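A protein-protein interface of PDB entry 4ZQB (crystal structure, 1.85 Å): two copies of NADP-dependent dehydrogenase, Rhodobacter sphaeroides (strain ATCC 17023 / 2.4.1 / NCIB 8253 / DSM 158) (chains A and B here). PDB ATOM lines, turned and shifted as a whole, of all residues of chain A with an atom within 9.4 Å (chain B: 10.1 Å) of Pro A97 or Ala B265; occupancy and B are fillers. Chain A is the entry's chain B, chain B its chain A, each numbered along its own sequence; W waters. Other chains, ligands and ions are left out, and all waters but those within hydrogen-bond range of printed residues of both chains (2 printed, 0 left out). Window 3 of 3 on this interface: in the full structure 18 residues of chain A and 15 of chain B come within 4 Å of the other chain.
The indole nitrogen (NE1) of Trp B269 is in hydrogen-bond range of the backbone carbonyl oxygen (O) of Pro B263 (3.0 Å).
Water W1 bridges the side-chain carboxylate (OE2) of Glu B264 (2.7 Å) and the backbone carbonyl oxygen (O) of Pro A308 (3.2 Å). Water W2 lies within hydrogen-bond range of the side-chain carboxylate (OE2) of Glu A150 (3.0 Å), the side-chain carboxylate (OE1) of Glu B264 (3.0 Å) and the guanidinium group (NH2) of Arg A93 (3.1 Å).
OE2 of Glu A150 lies within hydrogen-bond range of N of Glu B264 (2.9 Å). OE1 of Glu A150 sits at hydrogen-bond distance from N of Ala B265 (2.9 Å).
Printed residues of chain B that touch a printed residue of chain A: Pro B263, Glu B264 and Ala B265. Along chain B the printed residues that touch a printed residue of chain A span positions 263 to 265. Among the printed residues, 7 pairs touch across the chains.
No position is printed for both chains.
Val A95 touches Glu B264 (CG2 to OE2, 3.7 Å). N of Ala B265 touches CG1 of Val A95 (3.6 Å). Pro A97 touches Ala B265 (CG to O, 3.9 Å). Pro B263 touches Glu A150 (CB to OE1, 3.5 Å). Pro A308 touches Glu B264 (CG to OE2, 3.7 Å).
Pro A97 touches just one residue of chain B: Ala B265 (3.9 Å). Of chain A, only Val A95, Pro A97 and Glu A150 come within 4 Å of Ala B265. No residue of chain B comes within 4 Å of Asp A96. No residue of chain B comes within 4 Å of Ala A100. No residue of chain A comes within 4 Å of Ser B266. Of the printed residues of chain B, Val A95 touches Glu B264 and Ala B265. Printed residues of chain A within 4 Å of Pro B263: Glu A150. Of the printed residues of chain A, Glu B264 touches Val A95, Glu A150 and Pro A308. Of the printed residues of chain B, Pro A308 touches Glu B264 (3.7 Å). Of the printed residues of chain B, Glu A150 touches Pro B263 (3.5 Å), Glu B264 (2.9 Å) and Ala B265 (2.9 Å). Ala A154 touches none of the printed residues of chain B.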
ATOM      1  N   ARG A  93       4.394 -18.749  -4.223  1.00  0.00           N
ATOM      2  CA  ARG A  93       4.605 -18.894  -5.662  1.00  0.00           C
ATOM      3  C   ARG A  93       5.180 -20.288  -5.910  1.00  0.00           C
ATOM      4  O   ARG A  93       5.532 -20.972  -4.955  1.00  0.00           O
ATOM      5  CB  ARG A  93       5.486 -17.759  -6.169  1.00  0.00           C
ATOM      6  CG  ARG A  93       6.962 -17.954  -5.925  1.00  0.00           C
ATOM      7  CD  ARG A  93       7.725 -16.650  -5.828  1.00  0.00           C
ATOM      8  NE  ARG A  93       9.142 -16.940  -5.625  1.00  0.00           N
ATOM      9  CZ  ARG A  93       9.994 -17.207  -6.599  1.00  0.00           C
ATOM     10  NH1 ARG A  93       9.590 -17.238  -7.862  1.00  0.00           N
ATOM     11  NH2 ARG A  93      11.259 -17.439  -6.310  1.00  0.00           N
ATOM     12  N   LEU A  94       5.339 -20.678  -7.170  1.00  0.00           N
ATOM     13  CA  LEU A  94       6.015 -21.917  -7.478  1.00  0.00           C
ATOM     14  C   LEU A  94       7.539 -21.748  -7.472  1.00  0.00           C
ATOM     15  O   LEU A  94       8.098 -20.963  -8.245  1.00  0.00           O
ATOM     16  CB  LEU A  94       5.551 -22.491  -8.823  1.00  0.00           C
ATOM     17  CG  LEU A  94       6.218 -23.819  -9.181  1.00  0.00           C
ATOM     18  CD1 LEU A  94       5.758 -24.938  -8.238  1.00  0.00           C
ATOM     19  CD2 LEU A  94       6.011 -24.215 -10.642  1.00  0.00           C
ATOM     20  N   VAL A  95       8.187 -22.528  -6.607  1.00  0.00           N
ATOM     21  CA  VAL A  95       9.633 -22.741  -6.582  1.00  0.00           C
ATOM     22  C   VAL A  95       9.830 -24.254  -6.760  1.00  0.00           C
ATOM     23  O   VAL A  95       9.319 -25.038  -5.979  1.00  0.00           O
ATOM     24  CB  VAL A  95      10.236 -22.283  -5.234  1.00  0.00           C
ATOM     25  CG1 VAL A  95      11.727 -22.596  -5.165  1.00  0.00           C
ATOM     26  CG2 VAL A  95       9.981 -20.790  -5.010  1.00  0.00           C
ATOM     27  N   ASP A  96      10.521 -24.635  -7.830  1.00  0.00           N
ATOM     28  CA  ASP A  96      10.567 -26.022  -8.320  1.00  0.00           C
ATOM     29  C   ASP A  96      11.906 -26.238  -8.975  1.00  0.00           C
ATOM     30  O   ASP A  96      12.227 -25.544  -9.954  1.00  0.00           O
ATOM     31  CB  ASP A  96       9.433 -26.242  -9.348  1.00  0.00           C
ATOM     32  CG  ASP A  96       9.349 -27.685  -9.910  1.00  0.00           C
ATOM     33  OD1 ASP A  96      10.261 -28.556  -9.683  1.00  0.00           O
ATOM     34  OD2 ASP A  96       8.305 -27.956 -10.590  1.00  0.00           O
ATOM     35  N   PRO A  97      12.694 -27.207  -8.477  1.00  0.00           N
ATOM     36  CA  PRO A  97      13.979 -27.497  -9.134  1.00  0.00           C
ATOM     37  C   PRO A  97      13.867 -27.822 -10.615  1.00  0.00           C
ATOM     38  O   PRO A  97      14.781 -27.484 -11.394  1.00  0.00           O
ATOM     39  CB  PRO A  97      14.514 -28.745  -8.406  1.00  0.00           C
ATOM     40  CG  PRO A  97      13.596 -29.026  -7.293  1.00  0.00           C
ATOM     41  CD  PRO A  97      12.448 -28.081  -7.306  1.00  0.00           C
ATOM     42  N   GLU A  98      12.784 -28.470 -11.020  1.00  0.00           N
ATOM     43  CA  GLU A  98      12.581 -28.779 -12.426  1.00  0.00           C
ATOM     44  C   GLU A  98      12.353 -27.510 -13.287  1.00  0.00           C
ATOM     45  O   GLU A  98      12.746 -27.470 -14.441  1.00  0.00           O
ATOM     46  CB  GLU A  98      11.445 -29.796 -12.598  1.00  0.00           C
ATOM     47  CG  GLU A  98      11.126 -30.206 -14.030  1.00  0.00           C
ATOM     48  CD  GLU A  98      12.329 -30.616 -14.887  1.00  0.00           C
ATOM     49  OE1 GLU A  98      13.375 -30.990 -14.362  1.00  0.00           O
ATOM     50  OE2 GLU A  98      12.230 -30.609 -16.115  1.00  0.00           O
ATOM     51  N   LEU A  99      11.657 -26.520 -12.726  1.00  0.00           N
ATOM     52  CA  LEU A  99      11.492 -25.228 -13.389  1.00  0.00           C
ATOM     53  C   LEU A  99      12.847 -24.535 -13.532  1.00  0.00           C
ATOM     54  O   LEU A  99      13.155 -24.009 -14.603  1.00  0.00           O
ATOM     55  CB  LEU A  99      10.531 -24.332 -12.606  1.00  0.00           C
ATOM     56  CG  LEU A  99      10.123 -23.070 -13.338  1.00  0.00           C
ATOM     57  CD1 LEU A  99       9.244 -23.429 -14.543  1.00  0.00           C
ATOM     58  CD2 LEU A  99       9.392 -22.121 -12.380  1.00  0.00           C
ATOM     59  N   ALA A 100      13.638 -24.539 -12.468  1.00  0.00           N
ATOM     60  CA  ALA A 100      15.000 -23.986 -12.526  1.00  0.00           C
ATOM     61  C   ALA A 100      15.846 -24.676 -13.609  1.00  0.00           C
ATOM     62  O   ALA A 100      16.529 -24.001 -14.422  1.00  0.00           O
ATOM     63  CB  ALA A 100      15.671 -24.051 -11.165  1.00  0.00           C
ATOM     64  N   ARG A 101      15.796 -25.998 -13.645  1.00  0.00           N
ATOM     65  CA  ARG A 101      16.565 -26.788 -14.610  1.00  0.00           C
ATOM     66  C   ARG A 101      16.181 -26.437 -16.045  1.00  0.00           C
ATOM     67  O   ARG A 101      17.041 -26.223 -16.910  1.00  0.00           O
ATOM     68  CB  ARG A 101      16.398 -28.288 -14.369  1.00  0.00           C
ATOM     69  CG  ARG A 101      17.359 -29.170 -15.144  1.00  0.00           C
ATOM     70  CD  ARG A 101      16.803 -30.571 -15.450  1.00  0.00           C
ATOM     71  NE  ARG A 101      15.609 -30.494 -16.264  1.00  0.00           N
ATOM     72  CZ  ARG A 101      15.573 -30.176 -17.547  1.00  0.00           C
ATOM     73  NH1 ARG A 101      16.685 -30.008 -18.241  1.00  0.00           N
ATOM     74  NH2 ARG A 101      14.398 -30.070 -18.149  1.00  0.00           N
ATOM     75  N   THR A 102      14.863 -26.352 -16.265  1.00  0.00           N
ATOM     76  CA  THR A 102      14.313 -26.062 -17.573  1.00  0.00           C
ATOM     77  C   THR A 102      14.687 -24.647 -18.055  1.00  0.00           C
ATOM     78  O   THR A 102      15.079 -24.486 -19.211  1.00  0.00           O
ATOM     79  CB  THR A 102      12.796 -26.287 -17.577  1.00  0.00           C
ATOM     80  OG1 THR A 102      12.518 -27.638 -17.185  1.00  0.00           O
ATOM     81  CG2 THR A 102      12.215 -26.066 -18.937  1.00  0.00           C
ATOM     82  N   MET A 103      14.574 -23.643 -17.174  1.00  0.00           N
ATOM     83  CA  MET A 103      14.944 -22.278 -17.494  1.00  0.00           C
ATOM     84  C   MET A 103      16.443 -22.119 -17.704  1.00  0.00           C
ATOM     85  O   MET A 103      16.877 -21.393 -18.621  1.00  0.00           O
ATOM     86  CB  MET A 103      14.462 -21.275 -16.426  1.00  0.00           C
ATOM     87  CG  MET A 103      14.741 -19.802 -16.824  1.00  0.00           C
ATOM     88  SD  MET A 103      13.999 -19.339 -18.394  1.00  0.00           S
ATOM     89  CE  MET A 103      12.429 -18.661 -17.791  1.00  0.00           C
ATOM     90  N   ALA A 104      17.260 -22.775 -16.877  1.00  0.00           N
ATOM     91  CA  ALA A 104      18.699 -22.670 -17.047  1.00  0.00           C
ATOM     92  C   ALA A 104      19.102 -23.249 -18.424  1.00  0.00           C
ATOM     93  O   ALA A 104      19.974 -22.702 -19.108  1.00  0.00           O
ATOM     94  CB  ALA A 104      19.425 -23.400 -15.926  1.00  0.00           C
ATOM     95  N   GLU A 105      18.489 -24.383 -18.779  1.00  0.00           N
ATOM     96  CA  GLU A 105      18.623 -24.965 -20.107  1.00  0.00           C
ATOM     97  C   GLU A 105      18.227 -23.992 -21.210  1.00  0.00           C
ATOM     98  O   GLU A 105      18.971 -23.802 -22.181  1.00  0.00           O
ATOM     99  CB  GLU A 105      17.778 -26.239 -20.206  1.00  0.00           C
ATOM    100  CG  GLU A 105      17.644 -26.854 -21.598  1.00  0.00           C
ATOM    101  CD  GLU A 105      16.669 -28.011 -21.597  1.00  0.00           C
ATOM    102  OE1 GLU A 105      17.031 -29.083 -21.044  1.00  0.00           O
ATOM    103  OE2 GLU A 105      15.521 -27.834 -22.090  1.00  0.00           O
ATOM    104  N   GLY A 149      18.061 -15.386  -9.019  1.00  0.00           N
ATOM    105  CA  GLY A 149      17.124 -16.015  -8.116  1.00  0.00           C
ATOM    106  C   GLY A 149      17.062 -17.479  -8.420  1.00  0.00           C
ATOM    107  O   GLY A 149      18.042 -18.095  -8.850  1.00  0.00           O
ATOM    108  N   GLU A 150      15.917 -18.066  -8.142  1.00  0.00           N
ATOM    109  CA  GLU A 150      15.740 -19.513  -8.394  1.00  0.00           C
ATOM    110  C   GLU A 150      16.059 -19.878  -9.830  1.00  0.00           C
ATOM    111  O   GLU A 150      16.699 -20.886 -10.086  1.00  0.00           O
ATOM    112  CB  GLU A 150      14.314 -19.934  -8.076  1.00  0.00           C
ATOM    113  CG  GLU A 150      13.905 -19.705  -6.635  1.00  0.00           C
ATOM    114  CD  GLU A 150      14.829 -20.361  -5.621  1.00  0.00           C
ATOM    115  OE1 GLU A 150      15.268 -21.517  -5.850  1.00  0.00           O
ATOM    116  OE2 GLU A 150      15.129 -19.737  -4.588  1.00  0.00           O
ATOM    117  N   LEU A 151      15.685 -19.010 -10.770  1.00  0.00           N
ATOM    118  CA  LEU A 151      15.939 -19.284 -12.159  1.00  0.00           C
ATOM    119  C   LEU A 151      17.244 -18.667 -12.652  1.00  0.00           C
ATOM    120  O   LEU A 151      18.058 -19.358 -13.313  1.00  0.00           O
ATOM    121  CB  LEU A 151      14.758 -18.828 -13.011  1.00  0.00           C
ATOM    122  CG  LEU A 151      13.397 -19.316 -12.581  1.00  0.00           C
ATOM    123  CD1 LEU A 151      12.303 -18.857 -13.553  1.00  0.00           C
ATOM    124  CD2 LEU A 151      13.316 -20.816 -12.408  1.00  0.00           C
ATOM    125  N   ALA A 154      20.498 -20.442 -11.435  1.00  0.00           N
ATOM    126  CA  ALA A 154      20.617 -21.688 -12.170  1.00  0.00           C
ATOM    127  C   ALA A 154      21.110 -21.440 -13.587  1.00  0.00           C
ATOM    128  O   ALA A 154      21.968 -22.167 -14.079  1.00  0.00           O
ATOM    129  CB  ALA A 154      19.307 -22.481 -12.151  1.00  0.00           C
ATOM    130  N   ALA A 282      10.419 -21.630 -20.122  1.00  0.00           N
ATOM    131  CA  ALA A 282      10.267 -22.546 -18.978  1.00  0.00           C
ATOM    132  C   ALA A 282       8.810 -22.707 -18.578  1.00  0.00           C
ATOM    133  O   ALA A 282       8.334 -22.029 -17.689  1.00  0.00           O
ATOM    134  CB  ALA A 282      11.083 -22.076 -17.790  1.00  0.00           C
ATOM    135  N   ASP A 285       5.824 -27.567 -15.218  1.00  0.00           N
ATOM    136  CA  ASP A 285       5.576 -29.000 -15.374  1.00  0.00           C
ATOM    137  C   ASP A 285       4.469 -29.352 -14.348  1.00  0.00           C
ATOM    138  O   ASP A 285       4.712 -29.290 -13.151  1.00  0.00           O
ATOM    139  CB  ASP A 285       6.893 -29.737 -15.097  1.00  0.00           C
ATOM    140  CG  ASP A 285       6.780 -31.249 -15.153  1.00  0.00           C
ATOM    141  OD1 ASP A 285       5.806 -31.815 -14.679  1.00  0.00           O
ATOM    142  OD2 ASP A 285       7.729 -31.901 -15.627  1.00  0.00           O
ATOM    143  N   THR A 288       5.570 -32.182 -11.580  1.00  0.00           N
ATOM    144  CA  THR A 288       6.491 -31.798 -10.521  1.00  0.00           C
ATOM    145  C   THR A 288       5.869 -30.679  -9.663  1.00  0.00           C
ATOM    146  O   THR A 288       6.029 -30.676  -8.445  1.00  0.00           O
ATOM    147  CB  THR A 288       7.890 -31.360 -11.039  1.00  0.00           C
ATOM    148  OG1 THR A 288       7.779 -30.296 -11.971  1.00  0.00           O
ATOM    149  CG2 THR A 288       8.645 -32.536 -11.731  1.00  0.00           C
ATOM    150  N   ALA A 289       5.191 -29.721 -10.307  1.00  0.00           N
ATOM    151  CA  ALA A 289       4.565 -28.640  -9.554  1.00  0.00           C
ATOM    152  C   ALA A 289       3.487 -29.169  -8.613  1.00  0.00           C
ATOM    153  O   ALA A 289       3.403 -28.748  -7.444  1.00  0.00           O
ATOM    154  CB  ALA A 289       4.000 -27.569 -10.489  1.00  0.00           C
ATOM    155  N   ALA A 291       3.339 -32.130  -7.207  1.00  0.00           N
ATOM    156  CA  ALA A 291       4.021 -32.819  -6.086  1.00  0.00           C
ATOM    157  C   ALA A 291       4.562 -31.813  -5.063  1.00  0.00           C
ATOM    158  O   ALA A 291       4.556 -32.064  -3.870  1.00  0.00           O
ATOM    159  CB  ALA A 291       5.135 -33.704  -6.606  1.00  0.00           C
ATOM    160  N   ILE A 292       5.030 -30.673  -5.537  1.00  0.00           N
ATOM    161  CA  ILE A 292       5.472 -29.622  -4.629  1.00  0.00           C
ATOM    162  C   ILE A 292       4.302 -29.004  -3.811  1.00  0.00           C
ATOM    163  O   ILE A 292       4.395 -28.820  -2.589  1.00  0.00           O
ATOM    164  CB  ILE A 292       6.242 -28.550  -5.404  1.00  0.00           C
ATOM    165  CG1 ILE A 292       7.625 -29.133  -5.747  1.00  0.00           C
ATOM    166  CG2 ILE A 292       6.412 -27.278  -4.583  1.00  0.00           C
ATOM    167  CD1 ILE A 292       8.317 -28.374  -6.821  1.00  0.00           C
ATOM    168  N   HIS A 296       3.750 -29.273   0.326  1.00  0.00           N
ATOM    169  CA  HIS A 296       3.478 -28.064   1.096  1.00  0.00           C
ATOM    170  C   HIS A 296       2.189 -28.171   1.874  1.00  0.00           C
ATOM    171  O   HIS A 296       2.148 -27.796   3.048  1.00  0.00           O
ATOM    172  CB  HIS A 296       3.432 -26.852   0.159  1.00  0.00           C
ATOM    173  CG  HIS A 296       4.775 -26.359  -0.263  1.00  0.00           C
ATOM    174  ND1 HIS A 296       4.941 -25.542  -1.355  1.00  0.00           N
ATOM    175  CD2 HIS A 296       6.005 -26.528   0.266  1.00  0.00           C
ATOM    176  CE1 HIS A 296       6.215 -25.239  -1.494  1.00  0.00           C
ATOM    177  NE2 HIS A 296       6.878 -25.809  -0.510  1.00  0.00           N
ATOM    178  N   PRO A 308       7.429 -20.472   2.482  1.00  0.00           N
ATOM    179  CA  PRO A 308       7.859 -19.100   2.230  1.00  0.00           C
ATOM    180  C   PRO A 308       6.929 -18.387   1.266  1.00  0.00           C
ATOM    181  O   PRO A 308       6.485 -18.985   0.301  1.00  0.00           O
ATOM    182  CB  PRO A 308       9.245 -19.272   1.604  1.00  0.00           C
ATOM    183  CG  PRO A 308       9.737 -20.527   2.158  1.00  0.00           C
ATOM    184  CD  PRO A 308       8.534 -21.423   2.269  1.00  0.00           C
ATOM    185  N   ILE B 241      23.307 -36.382  -2.717  1.00  0.00           N
ATOM    186  CA  ILE B 241      21.890 -36.717  -2.511  1.00  0.00           C
ATOM    187  C   ILE B 241      21.630 -38.192  -2.806  1.00  0.00           C
ATOM    188  O   ILE B 241      20.936 -38.880  -2.018  1.00  0.00           O
ATOM    189  CB  ILE B 241      20.942 -35.856  -3.376  1.00  0.00           C
ATOM    190  CG1 ILE B 241      21.019 -34.386  -2.971  1.00  0.00           C
ATOM    191  CG2 ILE B 241      19.503 -36.392  -3.316  1.00  0.00           C
ATOM    192  CD1 ILE B 241      20.351 -34.066  -1.666  1.00  0.00           C
ATOM    193  N   VAL B 259      25.982 -21.665  -4.595  1.00  0.00           N
ATOM    194  CA  VAL B 259      25.253 -20.403  -4.583  1.00  0.00           C
ATOM    195  C   VAL B 259      24.837 -20.098  -3.132  1.00  0.00           C
ATOM    196  O   VAL B 259      24.242 -20.958  -2.460  1.00  0.00           O
ATOM    197  CB  VAL B 259      23.997 -20.498  -5.458  1.00  0.00           C
ATOM    198  CG1 VAL B 259      23.235 -19.178  -5.436  1.00  0.00           C
ATOM    199  CG2 VAL B 259      24.362 -20.906  -6.882  1.00  0.00           C
ATOM    200  N   PRO B 261      23.184 -16.714  -0.821  1.00  0.00           N
ATOM    201  CA  PRO B 261      22.378 -17.651   0.017  1.00  0.00           C
ATOM    202  C   PRO B 261      21.838 -18.831  -0.772  1.00  0.00           C
ATOM    203  O   PRO B 261      21.533 -18.710  -1.966  1.00  0.00           O
ATOM    204  CB  PRO B 261      21.223 -16.784   0.510  1.00  0.00           C
ATOM    205  CG  PRO B 261      21.706 -15.365   0.366  1.00  0.00           C
ATOM    206  CD  PRO B 261      22.642 -15.352  -0.815  1.00  0.00           C
ATOM    207  N   LEU B 262      21.761 -19.972  -0.110  1.00  0.00           N
ATOM    208  CA  LEU B 262      21.278 -21.209  -0.718  1.00  0.00           C
ATOM    209  C   LEU B 262      19.908 -20.976  -1.308  1.00  0.00           C
ATOM    210  O   LEU B 262      18.989 -20.556  -0.569  1.00  0.00           O
ATOM    211  CB  LEU B 262      21.212 -22.340   0.317  1.00  0.00           C
ATOM    212  CG  LEU B 262      20.815 -23.719  -0.180  1.00  0.00           C
ATOM    213  CD1 LEU B 262      21.833 -24.237  -1.195  1.00  0.00           C
ATOM    214  CD2 LEU B 262      20.713 -24.688   0.994  1.00  0.00           C
ATOM    215  N   PRO B 263      19.757 -21.204  -2.641  1.00  0.00           N
ATOM    216  CA  PRO B 263      18.408 -21.025  -3.211  1.00  0.00           C
ATOM    217  C   PRO B 263      17.339 -21.876  -2.523  1.00  0.00           C
ATOM    218  O   PRO B 263      17.588 -23.010  -2.122  1.00  0.00           O
ATOM    219  CB  PRO B 263      18.571 -21.474  -4.662  1.00  0.00           C
ATOM    220  CG  PRO B 263      20.005 -21.213  -4.963  1.00  0.00           C
ATOM    221  CD  PRO B 263      20.725 -21.574  -3.677  1.00  0.00           C
ATOM    222  N   GLU B 264      16.145 -21.315  -2.443  1.00  0.00           N
ATOM    223  CA  GLU B 264      15.001 -21.990  -1.840  1.00  0.00           C
ATOM    224  C   GLU B 264      14.681 -23.375  -2.478  1.00  0.00           C
ATOM    225  O   GLU B 264      14.201 -24.264  -1.787  1.00  0.00           O
ATOM    226  CB  GLU B 264      13.784 -21.067  -1.928  1.00  0.00           C
ATOM    227  CG  GLU B 264      12.631 -21.499  -1.042  1.00  0.00           C
ATOM    228  CD  GLU B 264      11.348 -20.761  -1.368  1.00  0.00           C
ATOM    229  OE1 GLU B 264      11.385 -19.539  -1.662  1.00  0.00           O
ATOM    230  OE2 GLU B 264      10.304 -21.456  -1.363  1.00  0.00           O
ATOM    231  N   ALA B 265      14.931 -23.538  -3.767  1.00  0.00           N
ATOM    232  CA  ALA B 265      14.704 -24.814  -4.454  1.00  0.00           C
ATOM    233  C   ALA B 265      15.730 -25.887  -4.148  1.00  0.00           C
ATOM    234  O   ALA B 265      15.527 -27.010  -4.565  1.00  0.00           O
ATOM    235  CB  ALA B 265      14.646 -24.613  -5.971  1.00  0.00           C
ATOM    236  N   SER B 266      16.831 -25.569  -3.464  1.00  0.00           N
ATOM    237  CA  SER B 266      17.815 -26.591  -3.141  1.00  0.00           C
ATOM    238  C   SER B 266      17.159 -27.751  -2.376  1.00  0.00           C
ATOM    239  O   SER B 266      16.427 -27.509  -1.404  1.00  0.00           O
ATOM    240  CB  SER B 266      18.947 -26.056  -2.276  1.00  0.00           C
ATOM    241  OG  SER B 266      19.784 -27.114  -1.797  1.00  0.00           O
ATOM    242  N   PRO B 267      17.461 -28.990  -2.784  1.00  0.00           N
ATOM    243  CA  PRO B 267      16.968 -30.133  -1.994  1.00  0.00           C
ATOM    244  C   PRO B 267      17.561 -30.210  -0.588  1.00  0.00           C
ATOM    245  O   PRO B 267      17.024 -30.937   0.239  1.00  0.00           O
ATOM    246  CB  PRO B 267      17.412 -31.334  -2.812  1.00  0.00           C
ATOM    247  CG  PRO B 267      18.579 -30.855  -3.601  1.00  0.00           C
ATOM    248  CD  PRO B 267      18.306 -29.415  -3.920  1.00  0.00           C
ATOM    249  N   PHE B 268      18.656 -29.478  -0.318  1.00  0.00           N
ATOM    250  CA  PHE B 268      19.289 -29.570   0.991  1.00  0.00           C
ATOM    251  C   PHE B 268      18.416 -29.019   2.141  1.00  0.00           C
ATOM    252  O   PHE B 268      18.510 -29.499   3.264  1.00  0.00           O
ATOM    253  CB  PHE B 268      20.617 -28.850   1.005  1.00  0.00           C
ATOM    254  CG  PHE B 268      21.656 -29.474   0.124  1.00  0.00           C
ATOM    255  CD1 PHE B 268      21.834 -30.855   0.092  1.00  0.00           C
ATOM    256  CD2 PHE B 268      22.481 -28.677  -0.640  1.00  0.00           C
ATOM    257  CE1 PHE B 268      22.816 -31.419  -0.719  1.00  0.00           C
ATOM    258  CE2 PHE B 268      23.452 -29.222  -1.456  1.00  0.00           C
ATOM    259  CZ  PHE B 268      23.631 -30.612  -1.476  1.00  0.00           C
ATOM    260  N   TRP B 269      17.612 -27.995   1.881  1.00  0.00           N
ATOM    261  CA  TRP B 269      16.839 -27.393   2.973  1.00  0.00           C
ATOM    262  C   TRP B 269      15.905 -28.394   3.616  1.00  0.00           C
ATOM    263  O   TRP B 269      15.811 -28.471   4.867  1.00  0.00           O
ATOM    264  CB  TRP B 269      15.982 -26.238   2.463  1.00  0.00           C
ATOM    265  CG  TRP B 269      16.634 -25.011   2.095  1.00  0.00           C
ATOM    266  CD1 TRP B 269      16.743 -24.521   0.829  1.00  0.00           C
ATOM    267  CD2 TRP B 269      17.173 -23.985   2.978  1.00  0.00           C
ATOM    268  NE1 TRP B 269      17.372 -23.313   0.853  1.00  0.00           N
ATOM    269  CE2 TRP B 269      17.644 -22.951   2.148  1.00  0.00           C
ATOM    270  CE3 TRP B 269      17.341 -23.869   4.363  1.00  0.00           C
ATOM    271  CZ2 TRP B 269      18.231 -21.778   2.659  1.00  0.00           C
ATOM    272  CZ3 TRP B 269      17.945 -22.723   4.885  1.00  0.00           C
ATOM    273  CH2 TRP B 269      18.368 -21.670   4.022  1.00  0.00           C
ATOM    274  N   GLY B 270      15.210 -29.164   2.773  1.00  0.00           N
ATOM    275  CA  GLY B 270      14.214 -30.092   3.243  1.00  0.00           C
ATOM    276  C   GLY B 270      14.651 -31.518   3.459  1.00  0.00           C
ATOM    277  O   GLY B 270      13.843 -32.336   3.904  1.00  0.00           O
ATOM    278  N   HIS B 271      15.898 -31.847   3.132  1.00  0.00           N
ATOM    279  CA  HIS B 271      16.302 -33.251   3.186  1.00  0.00           C
ATOM    280  C   HIS B 271      16.409 -33.669   4.661  1.00  0.00           C
ATOM    281  O   HIS B 271      17.057 -32.987   5.435  1.00  0.00           O
ATOM    282  CB  HIS B 271      17.636 -33.489   2.487  1.00  0.00           C
ATOM    283  CG  HIS B 271      17.841 -34.911   2.080  1.00  0.00           C
ATOM    284  ND1 HIS B 271      18.197 -35.899   2.971  1.00  0.00           N
ATOM    285  CD2 HIS B 271      17.665 -35.521   0.892  1.00  0.00           C
ATOM    286  CE1 HIS B 271      18.280 -37.050   2.334  1.00  0.00           C
ATOM    287  NE2 HIS B 271      17.953 -36.844   1.069  1.00  0.00           N
HETATM  288  O   HOH W   1       7.610 -21.201  -1.678  1.00  0.00           O
HETATM  289  O   HOH W   2      12.909 -17.995  -3.692  1.00  0.00           O
